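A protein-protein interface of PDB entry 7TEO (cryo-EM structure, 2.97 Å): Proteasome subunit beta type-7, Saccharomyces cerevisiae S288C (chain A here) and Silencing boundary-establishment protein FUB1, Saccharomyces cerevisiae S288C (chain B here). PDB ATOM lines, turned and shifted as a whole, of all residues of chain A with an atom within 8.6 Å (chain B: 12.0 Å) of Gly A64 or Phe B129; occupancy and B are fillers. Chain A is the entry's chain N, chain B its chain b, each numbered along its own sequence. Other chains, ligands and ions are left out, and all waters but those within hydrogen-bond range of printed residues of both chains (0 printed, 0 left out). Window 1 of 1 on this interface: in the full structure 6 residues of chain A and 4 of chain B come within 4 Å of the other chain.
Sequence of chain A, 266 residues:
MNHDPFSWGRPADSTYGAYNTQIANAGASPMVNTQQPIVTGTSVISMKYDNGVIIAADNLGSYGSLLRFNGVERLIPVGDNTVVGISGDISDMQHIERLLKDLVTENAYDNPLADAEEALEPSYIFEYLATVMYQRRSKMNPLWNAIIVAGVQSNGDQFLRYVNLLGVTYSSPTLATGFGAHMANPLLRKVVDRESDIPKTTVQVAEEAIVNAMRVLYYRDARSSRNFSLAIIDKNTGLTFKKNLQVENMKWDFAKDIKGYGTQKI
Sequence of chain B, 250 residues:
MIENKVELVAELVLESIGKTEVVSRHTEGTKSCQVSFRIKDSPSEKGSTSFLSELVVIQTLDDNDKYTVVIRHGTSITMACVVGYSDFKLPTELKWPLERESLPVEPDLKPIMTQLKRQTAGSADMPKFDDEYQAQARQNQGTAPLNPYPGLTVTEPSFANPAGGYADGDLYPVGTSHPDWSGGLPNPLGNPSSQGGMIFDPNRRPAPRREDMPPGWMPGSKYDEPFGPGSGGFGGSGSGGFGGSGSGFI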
ATOM      1  N   PRO A  37      20.517  -4.064   3.140  1.00  0.00           N
ATOM      2  CA  PRO A  37      21.715  -4.870   3.393  1.00  0.00           C
ATOM      3  C   PRO A  37      21.547  -5.719   4.643  1.00  0.00           C
ATOM      4  O   PRO A  37      20.850  -5.337   5.588  1.00  0.00           O
ATOM      5  CB  PRO A  37      22.810  -3.816   3.569  1.00  0.00           C
ATOM      6  CG  PRO A  37      22.092  -2.662   4.173  1.00  0.00           C
ATOM      7  CD  PRO A  37      20.698  -2.670   3.585  1.00  0.00           C
ATOM      8  N   ILE A  38      22.195  -6.883   4.645  1.00  0.00           N
ATOM      9  CA  ILE A  38      22.030  -7.848   5.728  1.00  0.00           C
ATOM     10  C   ILE A  38      23.369  -8.084   6.415  1.00  0.00           C
ATOM     11  O   ILE A  38      23.513  -7.825   7.614  1.00  0.00           O
ATOM     12  CB  ILE A  38      21.420  -9.157   5.199  1.00  0.00           C
ATOM     13  CG1 ILE A  38      20.007  -8.877   4.676  1.00  0.00           C
ATOM     14  CG2 ILE A  38      21.389 -10.214   6.297  1.00  0.00           C
ATOM     15  CD1 ILE A  38      19.358 -10.023   3.936  1.00  0.00           C
ATOM     16  N   VAL A  39      24.356  -8.570   5.665  1.00  0.00           N
ATOM     17  CA  VAL A  39      25.722  -8.731   6.154  1.00  0.00           C
ATOM     18  C   VAL A  39      26.575  -7.672   5.475  1.00  0.00           C
ATOM     19  O   VAL A  39      26.619  -7.602   4.241  1.00  0.00           O
ATOM     20  CB  VAL A  39      26.265 -10.143   5.873  1.00  0.00           C
ATOM     21  CG1 VAL A  39      27.693 -10.270   6.369  1.00  0.00           C
ATOM     22  CG2 VAL A  39      25.381 -11.199   6.517  1.00  0.00           C
ATOM     23  N   THR A  40      27.255  -6.850   6.273  1.00  0.00           N
ATOM     24  CA  THR A  40      27.893  -5.640   5.774  1.00  0.00           C
ATOM     25  C   THR A  40      29.326  -5.522   6.270  1.00  0.00           C
ATOM     26  O   THR A  40      29.655  -5.983   7.365  1.00  0.00           O
ATOM     27  CB  THR A  40      27.117  -4.393   6.209  1.00  0.00           C
ATOM     28  OG1 THR A  40      27.120  -4.300   7.639  1.00  0.00           O
ATOM     29  CG2 THR A  40      25.685  -4.445   5.711  1.00  0.00           C
ATOM     30  N   THR A  42      31.956  -2.524   7.244  1.00  0.00           N
ATOM     31  CA  THR A  42      31.718  -1.160   7.706  1.00  0.00           C
ATOM     32  C   THR A  42      32.326  -0.076   6.817  1.00  0.00           C
ATOM     33  O   THR A  42      31.580   0.705   6.217  1.00  0.00           O
ATOM     34  CB  THR A  42      32.212  -1.008   9.153  1.00  0.00           C
ATOM     35  OG1 THR A  42      31.829   0.279   9.658  1.00  0.00           O
ATOM     36  CG2 THR A  42      33.722  -1.190   9.273  1.00  0.00           C
ATOM     37  N   LEU A  60      36.030  -7.539   8.928  1.00  0.00           N
ATOM     38  CA  LEU A  60      34.851  -7.971   9.667  1.00  0.00           C
ATOM     39  C   LEU A  60      33.583  -7.699   8.869  1.00  0.00           C
ATOM     40  O   LEU A  60      33.345  -6.565   8.440  1.00  0.00           O
ATOM     41  CB  LEU A  60      34.781  -7.265  11.022  1.00  0.00           C
ATOM     42  CG  LEU A  60      33.460  -7.319  11.790  1.00  0.00           C
ATOM     43  CD1 LEU A  60      33.071  -8.747  12.106  1.00  0.00           C
ATOM     44  CD2 LEU A  60      33.569  -6.506  13.065  1.00  0.00           C
ATOM     45  N   GLY A  61      32.776  -8.741   8.678  1.00  0.00           N
ATOM     46  CA  GLY A  61      31.445  -8.604   8.133  1.00  0.00           C
ATOM     47  C   GLY A  61      30.417  -8.857   9.215  1.00  0.00           C
ATOM     48  O   GLY A  61      30.379  -9.938   9.806  1.00  0.00           O
ATOM     49  N   SER A  62      29.579  -7.857   9.469  1.00  0.00           N
ATOM     50  CA  SER A  62      28.671  -7.859  10.608  1.00  0.00           C
ATOM     51  C   SER A  62      27.249  -8.151  10.150  1.00  0.00           C
ATOM     52  O   SER A  62      26.756  -7.531   9.203  1.00  0.00           O
ATOM     53  CB  SER A  62      28.717  -6.519  11.341  1.00  0.00           C
ATOM     54  OG  SER A  62      29.980  -6.315  11.945  1.00  0.00           O
ATOM     55  N   TYR A  63      26.598  -9.086  10.835  1.00  0.00           N
ATOM     56  CA  TYR A  63      25.197  -9.431  10.596  1.00  0.00           C
ATOM     57  C   TYR A  63      24.370  -8.652  11.611  1.00  0.00           C
ATOM     58  O   TYR A  63      24.076  -9.136  12.704  1.00  0.00           O
ATOM     59  CB  TYR A  63      24.991 -10.935  10.722  1.00  0.00           C
ATOM     60  CG  TYR A  63      23.555 -11.384  10.595  1.00  0.00           C
ATOM     61  CD1 TYR A  63      22.955 -11.517   9.352  1.00  0.00           C
ATOM     62  CD2 TYR A  63      22.802 -11.681  11.722  1.00  0.00           C
ATOM     63  CE1 TYR A  63      21.644 -11.932   9.236  1.00  0.00           C
ATOM     64  CE2 TYR A  63      21.491 -12.094  11.615  1.00  0.00           C
ATOM     65  CZ  TYR A  63      20.916 -12.219  10.371  1.00  0.00           C
ATOM     66  OH  TYR A  63      19.608 -12.632  10.263  1.00  0.00           O
ATOM     67  N   GLY A  64      23.986  -7.435  11.243  1.00  0.00           N
ATOM     68  CA  GLY A  64      23.365  -6.551  12.214  1.00  0.00           C
ATOM     69  C   GLY A  64      24.386  -6.125  13.248  1.00  0.00           C
ATOM     70  O   GLY A  64      25.493  -5.689  12.913  1.00  0.00           O
ATOM     71  N   SER A  65      24.022  -6.239  14.523  1.00  0.00           N
ATOM     72  CA  SER A  65      24.966  -5.980  15.603  1.00  0.00           C
ATOM     73  C   SER A  65      25.812  -7.198  15.947  1.00  0.00           C
ATOM     74  O   SER A  65      26.688  -7.099  16.812  1.00  0.00           O
ATOM     75  CB  SER A  65      24.221  -5.504  16.853  1.00  0.00           C
ATOM     76  OG  SER A  65      23.381  -6.522  17.362  1.00  0.00           O
ATOM     77  N   LEU A  66      25.569  -8.334  15.300  1.00  0.00           N
ATOM     78  CA  LEU A  66      26.341  -9.545  15.544  1.00  0.00           C
ATOM     79  C   LEU A  66      27.597  -9.533  14.681  1.00  0.00           C
ATOM     80  O   LEU A  66      27.510  -9.582  13.451  1.00  0.00           O
ATOM     81  CB  LEU A  66      25.489 -10.776  15.241  1.00  0.00           C
ATOM     82  CG  LEU A  66      26.208 -12.124  15.183  1.00  0.00           C
ATOM     83  CD1 LEU A  66      27.032 -12.359  16.436  1.00  0.00           C
ATOM     84  CD2 LEU A  66      25.209 -13.247  14.975  1.00  0.00           C
ATOM     85  N   LEU A  67      28.764  -9.477  15.325  1.00  0.00           N
ATOM     86  CA  LEU A  67      30.045  -9.500  14.617  1.00  0.00           C
ATOM     87  C   LEU A  67      30.305 -10.931  14.140  1.00  0.00           C
ATOM     88  O   LEU A  67      31.115 -11.679  14.691  1.00  0.00           O
ATOM     89  CB  LEU A  67      31.159  -8.984  15.515  1.00  0.00           C
ATOM     90  CG  LEU A  67      30.861  -7.678  16.258  1.00  0.00           C
ATOM     91  CD1 LEU A  67      32.124  -7.126  16.895  1.00  0.00           C
ATOM     92  CD2 LEU A  67      30.228  -6.640  15.343  1.00  0.00           C
ATOM     93  N   ARG A  68      29.590 -11.300  13.076  1.00  0.00           N
ATOM     94  CA  ARG A  68      29.472 -12.707  12.706  1.00  0.00           C
ATOM     95  C   ARG A  68      30.732 -13.223  12.021  1.00  0.00           C
ATOM     96  O   ARG A  68      31.376 -14.157  12.512  1.00  0.00           O
ATOM     97  CB  ARG A  68      28.255 -12.896  11.800  1.00  0.00           C
ATOM     98  CG  ARG A  68      27.699 -14.304  11.801  1.00  0.00           C
ATOM     99  CD  ARG A  68      26.353 -14.356  11.110  1.00  0.00           C
ATOM    100  NE  ARG A  68      25.885 -15.724  10.930  1.00  0.00           N
ATOM    101  CZ  ARG A  68      24.683 -16.051  10.477  1.00  0.00           C
ATOM    102  NH1 ARG A  68      23.796 -15.131  10.140  1.00  0.00           N
ATOM    103  NH2 ARG A  68      24.365 -17.336  10.355  1.00  0.00           N
ATOM    104  N   PHE A 179      31.544   5.141   8.431  1.00  0.00           N
ATOM    105  CA  PHE A 179      32.064   5.969   9.513  1.00  0.00           C
ATOM    106  C   PHE A 179      33.421   6.571   9.180  1.00  0.00           C
ATOM    107  O   PHE A 179      33.818   7.556   9.808  1.00  0.00           O
ATOM    108  CB  PHE A 179      32.163   5.152  10.800  1.00  0.00           C
ATOM    109  CG  PHE A 179      30.987   5.325  11.708  1.00  0.00           C
ATOM    110  CD1 PHE A 179      29.759   4.786  11.376  1.00  0.00           C
ATOM    111  CD2 PHE A 179      31.105   6.041  12.884  1.00  0.00           C
ATOM    112  CE1 PHE A 179      28.671   4.949  12.204  1.00  0.00           C
ATOM    113  CE2 PHE A 179      30.021   6.209  13.715  1.00  0.00           C
ATOM    114  CZ  PHE A 179      28.801   5.660  13.373  1.00  0.00           C
ATOM    115  N   ASP A 221      34.018   3.085  16.144  1.00  0.00           N
ATOM    116  CA  ASP A 221      33.068   2.425  15.260  1.00  0.00           C
ATOM    117  C   ASP A 221      32.700   1.071  15.853  1.00  0.00           C
ATOM    118  O   ASP A 221      33.569   0.212  16.039  1.00  0.00           O
ATOM    119  CB  ASP A 221      33.650   2.262  13.857  1.00  0.00           C
ATOM    120  CG  ASP A 221      32.637   1.740  12.862  1.00  0.00           C
ATOM    121  OD1 ASP A 221      31.462   1.566  13.246  1.00  0.00           O
ATOM    122  OD2 ASP A 221      33.014   1.507  11.695  1.00  0.00           O
ATOM    123  N   ALA A 222      31.413   0.883  16.149  1.00  0.00           N
ATOM    124  CA  ALA A 222      30.959  -0.366  16.751  1.00  0.00           C
ATOM    125  C   ALA A 222      31.008  -1.531  15.774  1.00  0.00           C
ATOM    126  O   ALA A 222      31.059  -2.686  16.210  1.00  0.00           O
ATOM    127  CB  ALA A 222      29.538  -0.201  17.289  1.00  0.00           C
ATOM    128  N   ARG A 223      30.995  -1.259  14.473  1.00  0.00           N
ATOM    129  CA  ARG A 223      31.017  -2.295  13.452  1.00  0.00           C
ATOM    130  C   ARG A 223      32.427  -2.721  13.070  1.00  0.00           C
ATOM    131  O   ARG A 223      32.582  -3.628  12.246  1.00  0.00           O
ATOM    132  CB  ARG A 223      30.292  -1.801  12.197  1.00  0.00           C
ATOM    133  CG  ARG A 223      28.802  -1.588  12.374  1.00  0.00           C
ATOM    134  CD  ARG A 223      28.162  -1.134  11.075  1.00  0.00           C
ATOM    135  NE  ARG A 223      26.743  -0.831  11.233  1.00  0.00           N
ATOM    136  CZ  ARG A 223      25.764  -1.714  11.098  1.00  0.00           C
ATOM    137  NH1 ARG A 223      26.007  -2.985  10.820  1.00  0.00           N
ATOM    138  NH2 ARG A 223      24.505  -1.311  11.251  1.00  0.00           N
ATOM    139  N   SER A 224      33.452  -2.097  13.639  1.00  0.00           N
ATOM    140  CA  SER A 224      34.828  -2.295  13.215  1.00  0.00           C
ATOM    141  C   SER A 224      35.478  -3.445  13.975  1.00  0.00           C
ATOM    142  O   SER A 224      34.939  -3.961  14.956  1.00  0.00           O
ATOM    143  CB  SER A 224      35.641  -1.016  13.415  1.00  0.00           C
ATOM    144  OG  SER A 224      36.930  -1.138  12.843  1.00  0.00           O
ATOM    145  N   PRO B 127      19.210  -8.388  14.467  1.00  0.00           N
ATOM    146  CA  PRO B 127      19.817  -7.888  15.705  1.00  0.00           C
ATOM    147  C   PRO B 127      20.112  -6.392  15.655  1.00  0.00           C
ATOM    148  O   PRO B 127      20.960  -5.954  14.880  1.00  0.00           O
ATOM    149  CB  PRO B 127      21.111  -8.704  15.812  1.00  0.00           C
ATOM    150  CG  PRO B 127      20.828  -9.948  15.047  1.00  0.00           C
ATOM    151  CD  PRO B 127      19.980  -9.506  13.898  1.00  0.00           C
ATOM    152  N   LYS B 128      19.412  -5.619  16.481  1.00  0.00           N
ATOM    153  CA  LYS B 128      19.559  -4.173  16.482  1.00  0.00           C
ATOM    154  C   LYS B 128      20.670  -3.738  17.435  1.00  0.00           C
ATOM    155  O   LYS B 128      21.034  -4.448  18.377  1.00  0.00           O
ATOM    156  CB  LYS B 128      18.243  -3.503  16.879  1.00  0.00           C
ATOM    157  CG  LYS B 128      17.320  -3.191  15.707  1.00  0.00           C
ATOM    158  CD  LYS B 128      16.682  -4.445  15.122  1.00  0.00           C
ATOM    159  CE  LYS B 128      15.687  -5.078  16.086  1.00  0.00           C
ATOM    160  NZ  LYS B 128      14.834  -6.104  15.424  1.00  0.00           N
ATOM    161  N   PHE B 129      21.207  -2.548  17.177  1.00  0.00           N
ATOM    162  CA  PHE B 129      22.220  -1.967  18.043  1.00  0.00           C
ATOM    163  C   PHE B 129      21.578  -1.323  19.268  1.00  0.00           C
ATOM    164  O   PHE B 129      20.423  -0.891  19.245  1.00  0.00           O
ATOM    165  CB  PHE B 129      23.046  -0.922  17.293  1.00  0.00           C
ATOM    166  CG  PHE B 129      24.161  -1.500  16.470  1.00  0.00           C
ATOM    167  CD1 PHE B 129      25.395  -1.756  17.039  1.00  0.00           C
ATOM    168  CD2 PHE B 129      23.980  -1.773  15.125  1.00  0.00           C
ATOM    169  CE1 PHE B 129      26.424  -2.283  16.289  1.00  0.00           C
ATOM    170  CE2 PHE B 129      25.009  -2.300  14.371  1.00  0.00           C
ATOM    171  CZ  PHE B 129      26.233  -2.553  14.954  1.00  0.00           C
ATOM    172  N   ASP B 130      22.351  -1.264  20.349  1.00  0.00           N
ATOM    173  CA  ASP B 130      21.883  -0.613  21.564  1.00  0.00           C
ATOM    174  C   ASP B 130      21.919   0.901  21.406  1.00  0.00           C
ATOM    175  O   ASP B 130      22.860   1.463  20.840  1.00  0.00           O
ATOM    176  CB  ASP B 130      22.744  -1.031  22.757  1.00  0.00           C
ATOM    177  CG  ASP B 130      22.501  -2.467  23.177  1.00  0.00           C
ATOM    178  OD1 ASP B 130      21.370  -2.960  22.990  1.00  0.00           O
ATOM    179  OD2 ASP B 130      23.442  -3.101  23.701  1.00  0.00           O
ATOM    180  N   ASP B 131      20.879   1.563  21.914  1.00  0.00           N
ATOM    181  CA  ASP B 131      20.825   3.025  22.008  1.00  0.00           C
ATOM    182  C   ASP B 131      20.492   3.338  23.462  1.00  0.00           C
ATOM    183  O   ASP B 131      19.331   3.550  23.820  1.00  0.00           O
ATOM    184  CB  ASP B 131      19.802   3.612  21.037  1.00  0.00           C
ATOM    185  CG  ASP B 131      19.793   5.129  21.041  1.00  0.00           C
ATOM    186  OD1 ASP B 131      20.187   5.730  22.063  1.00  0.00           O
ATOM    187  OD2 ASP B 131      19.394   5.724  20.019  1.00  0.00           O
ATOM    188  N   GLU B 132      21.527   3.366  24.303  1.00  0.00           N
ATOM    189  CA  GLU B 132      21.311   3.529  25.736  1.00  0.00           C
ATOM    190  C   GLU B 132      20.810   4.928  26.068  1.00  0.00           C
ATOM    191  O   GLU B 132      19.961   5.095  26.950  1.00  0.00           O
ATOM    192  CB  GLU B 132      22.604   3.222  26.488  1.00  0.00           C
ATOM    193  CG  GLU B 132      22.944   1.739  26.543  1.00  0.00           C
ATOM    194  CD  GLU B 132      23.886   1.311  25.433  1.00  0.00           C
ATOM    195  OE1 GLU B 132      24.435   0.193  25.516  1.00  0.00           O
ATOM    196  OE2 GLU B 132      24.072   2.089  24.474  1.00  0.00           O
ATOM    197  N   TYR B 133      21.321   5.945  25.374  1.00  0.00           N
ATOM    198  CA  TYR B 133      20.909   7.317  25.641  1.00  0.00           C
ATOM    199  C   TYR B 133      19.583   7.671  24.987  1.00  0.00           C
ATOM    200  O   TYR B 133      19.078   8.774  25.221  1.00  0.00           O
ATOM    201  CB  TYR B 133      21.972   8.293  25.145  1.00  0.00           C
ATOM    202  CG  TYR B 133      23.362   7.989  25.641  1.00  0.00           C
ATOM    203  CD1 TYR B 133      23.617   7.786  26.989  1.00  0.00           C
ATOM    204  CD2 TYR B 133      24.423   7.911  24.753  1.00  0.00           C
ATOM    205  CE1 TYR B 133      24.892   7.506  27.433  1.00  0.00           C
ATOM    206  CE2 TYR B 133      25.696   7.636  25.187  1.00  0.00           C
ATOM    207  CZ  TYR B 133      25.928   7.432  26.525  1.00  0.00           C
ATOM    208  OH  TYR B 133      27.205   7.158  26.955  1.00  0.00           O
ATOM    209  N   GLN B 134      19.016   6.780  24.175  1.00  0.00           N
ATOM    210  CA  GLN B 134      17.842   7.083  23.365  1.00  0.00           C
ATOM    211  C   GLN B 134      18.118   8.207  22.374  1.00  0.00           C
ATOM    212  O   GLN B 134      17.194   8.907  21.949  1.00  0.00           O
ATOM    213  CB  GLN B 134      16.640   7.437  24.246  1.00  0.00           C
ATOM    214  CG  GLN B 134      16.460   6.516  25.441  1.00  0.00           C
ATOM    215  CD  GLN B 134      15.123   6.705  26.124  1.00  0.00           C
ATOM    216  OE1 GLN B 134      15.052   7.214  27.244  1.00  0.00           O
ATOM    217  NE2 GLN B 134      14.052   6.293  25.456  1.00  0.00           N
ATOM    218  N   ALA B 135      19.387   8.386  21.997  1.00  0.00           N
ATOM    219  CA  ALA B 135      19.753   9.479  21.104  1.00  0.00           C
ATOM    220  C   ALA B 135      19.064   9.362  19.752  1.00  0.00           C
ATOM    221  O   ALA B 135      18.617  10.371  19.195  1.00  0.00           O
ATOM    222  CB  ALA B 135      21.269   9.512  20.917  1.00  0.00           C
ATOM    223  N   GLN B 136      18.966   8.150  19.210  1.00  0.00           N
ATOM    224  CA  GLN B 136      18.310   7.925  17.931  1.00  0.00           C
ATOM    225  C   GLN B 136      16.831   7.607  18.091  1.00  0.00           C
ATOM    226  O   GLN B 136      16.159   7.317  17.095  1.00  0.00           O
ATOM    227  CB  GLN B 136      19.005   6.795  17.170  1.00  0.00           C
ATOM    228  CG  GLN B 136      20.494   7.011  16.964  1.00  0.00           C
ATOM    229  CD  GLN B 136      21.012   6.343  15.707  1.00  0.00           C
ATOM    230  OE1 GLN B 136      20.361   5.465  15.143  1.00  0.00           O
ATOM    231  NE2 GLN B 136      22.193   6.756  15.263  1.00  0.00           N
ATOM    232  N   ALA B 137      16.310   7.650  19.314  1.00  0.00           N
ATOM    233  CA  ALA B 137      14.883   7.452  19.521  1.00  0.00           C
ATOM    234  C   ALA B 137      14.107   8.540  18.794  1.00  0.00           C
ATOM    235  O   ALA B 137      14.417   9.729  18.920  1.00  0.00           O
ATOM    236  CB  ALA B 137      14.556   7.468  21.013  1.00  0.00           C
ATOM    237  N   ARG B 138      13.096   8.132  18.034  1.00  0.00           N
ATOM    238  CA  ARG B 138      12.306   9.040  17.220  1.00  0.00           C
ATOM    239  C   ARG B 138      10.881   9.100  17.752  1.00  0.00           C
ATOM    240  O   ARG B 138      10.328   8.094  18.208  1.00  0.00           O
ATOM    241  CB  ARG B 138      12.295   8.602  15.750  1.00  0.00           C
ATOM    242  CG  ARG B 138      13.664   8.226  15.198  1.00  0.00           C
ATOM    243  CD  ARG B 138      14.667   9.365  15.319  1.00  0.00           C
ATOM    244  NE  ARG B 138      15.973   8.997  14.787  1.00  0.00           N
ATOM    245  CZ  ARG B 138      17.045   9.777  14.821  1.00  0.00           C
ATOM    246  NH1 ARG B 138      17.003  10.988  15.350  1.00  0.00           N
ATOM    247  NH2 ARG B 138      18.189   9.330  14.310  1.00  0.00           N
ATOM    248  N   PRO B 229      25.771  12.415  11.980  1.00  0.00           N
ATOM    249  CA  PRO B 229      25.327  11.211  11.269  1.00  0.00           C
ATOM    250  C   PRO B 229      25.890   9.927  11.869  1.00  0.00           C
ATOM    251  O   PRO B 229      25.482   8.842  11.454  1.00  0.00           O
ATOM    252  CB  PRO B 229      25.859  11.432   9.853  1.00  0.00           C
ATOM    253  CG  PRO B 229      27.064  12.281  10.040  1.00  0.00           C
ATOM    254  CD  PRO B 229      26.765  13.178  11.205  1.00  0.00           C
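Phe B129 touches just these residues of chain A: Gly A64, Ser A65, Ala A222 and Arg A223. No residue of chain B comes within 4 Å of Thr A40. Tyr A63 touches one residue of chain B. Ser A65 touches just these residues of chain B: Pro B127 (3.1 Å), Lys B128 (3.3 Å) and Phe B129 (3.7 Å). No residue of chain B comes within 4 Å of Leu A66. Ala A222 touches just one residue of chain B: Phe B129 (3.9 Å). Arg A223 touches just one residue of chain B: Phe B129 (3.3 Å). Of the printed residues of chain A, Lys B128 touches Ser A65 (3.3 Å). Of the printed residues of chain A, Pro B127 touches Tyr A63, Gly A64 and Ser A65. Ala B137 touches none of the printed residues of chain A.
NH1 of Arg A223 is in hydrogen-bond range of O of Gly A64 (3.5 Å). OD1 of Asp A221 sits at hydrogen-bond distance from N of Arg A223 (3.1 Å).
The backbone NH of Ser A65 lies within hydrogen-bond range of the backbone carbonyl oxygen of Pro B127. The backbone carbonyl oxygen of Lys B128 is in hydrogen-bond range of the side-chain hydroxyl of Ser A65 (3.3 Å).
Of the 19 printed residues of chain A, 5 touch a printed residue of chain B. Printed residues of chain B that touch a printed residue of chain A: Pro B127, Lys B128 and Phe B129. Hydrophobic or aromatic side chains of chain B that line the printed part of chain A: Pro B127 and Phe B129. Among the printed residues, 8 pairs touch across the chains.
Pro B127 touches Tyr A63. Pro B127 touches Gly A64 (O to CA, 3.6 Å). Gly A64 touches Phe B129 (O to CE2, 3.7 Å). CA of Ser A65 touches CZ of Phe B129, 3.7 Å away. CE1 of Phe B129 touches CB of Ala A222 (3.9 Å). Phe B129 touches Arg A223.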
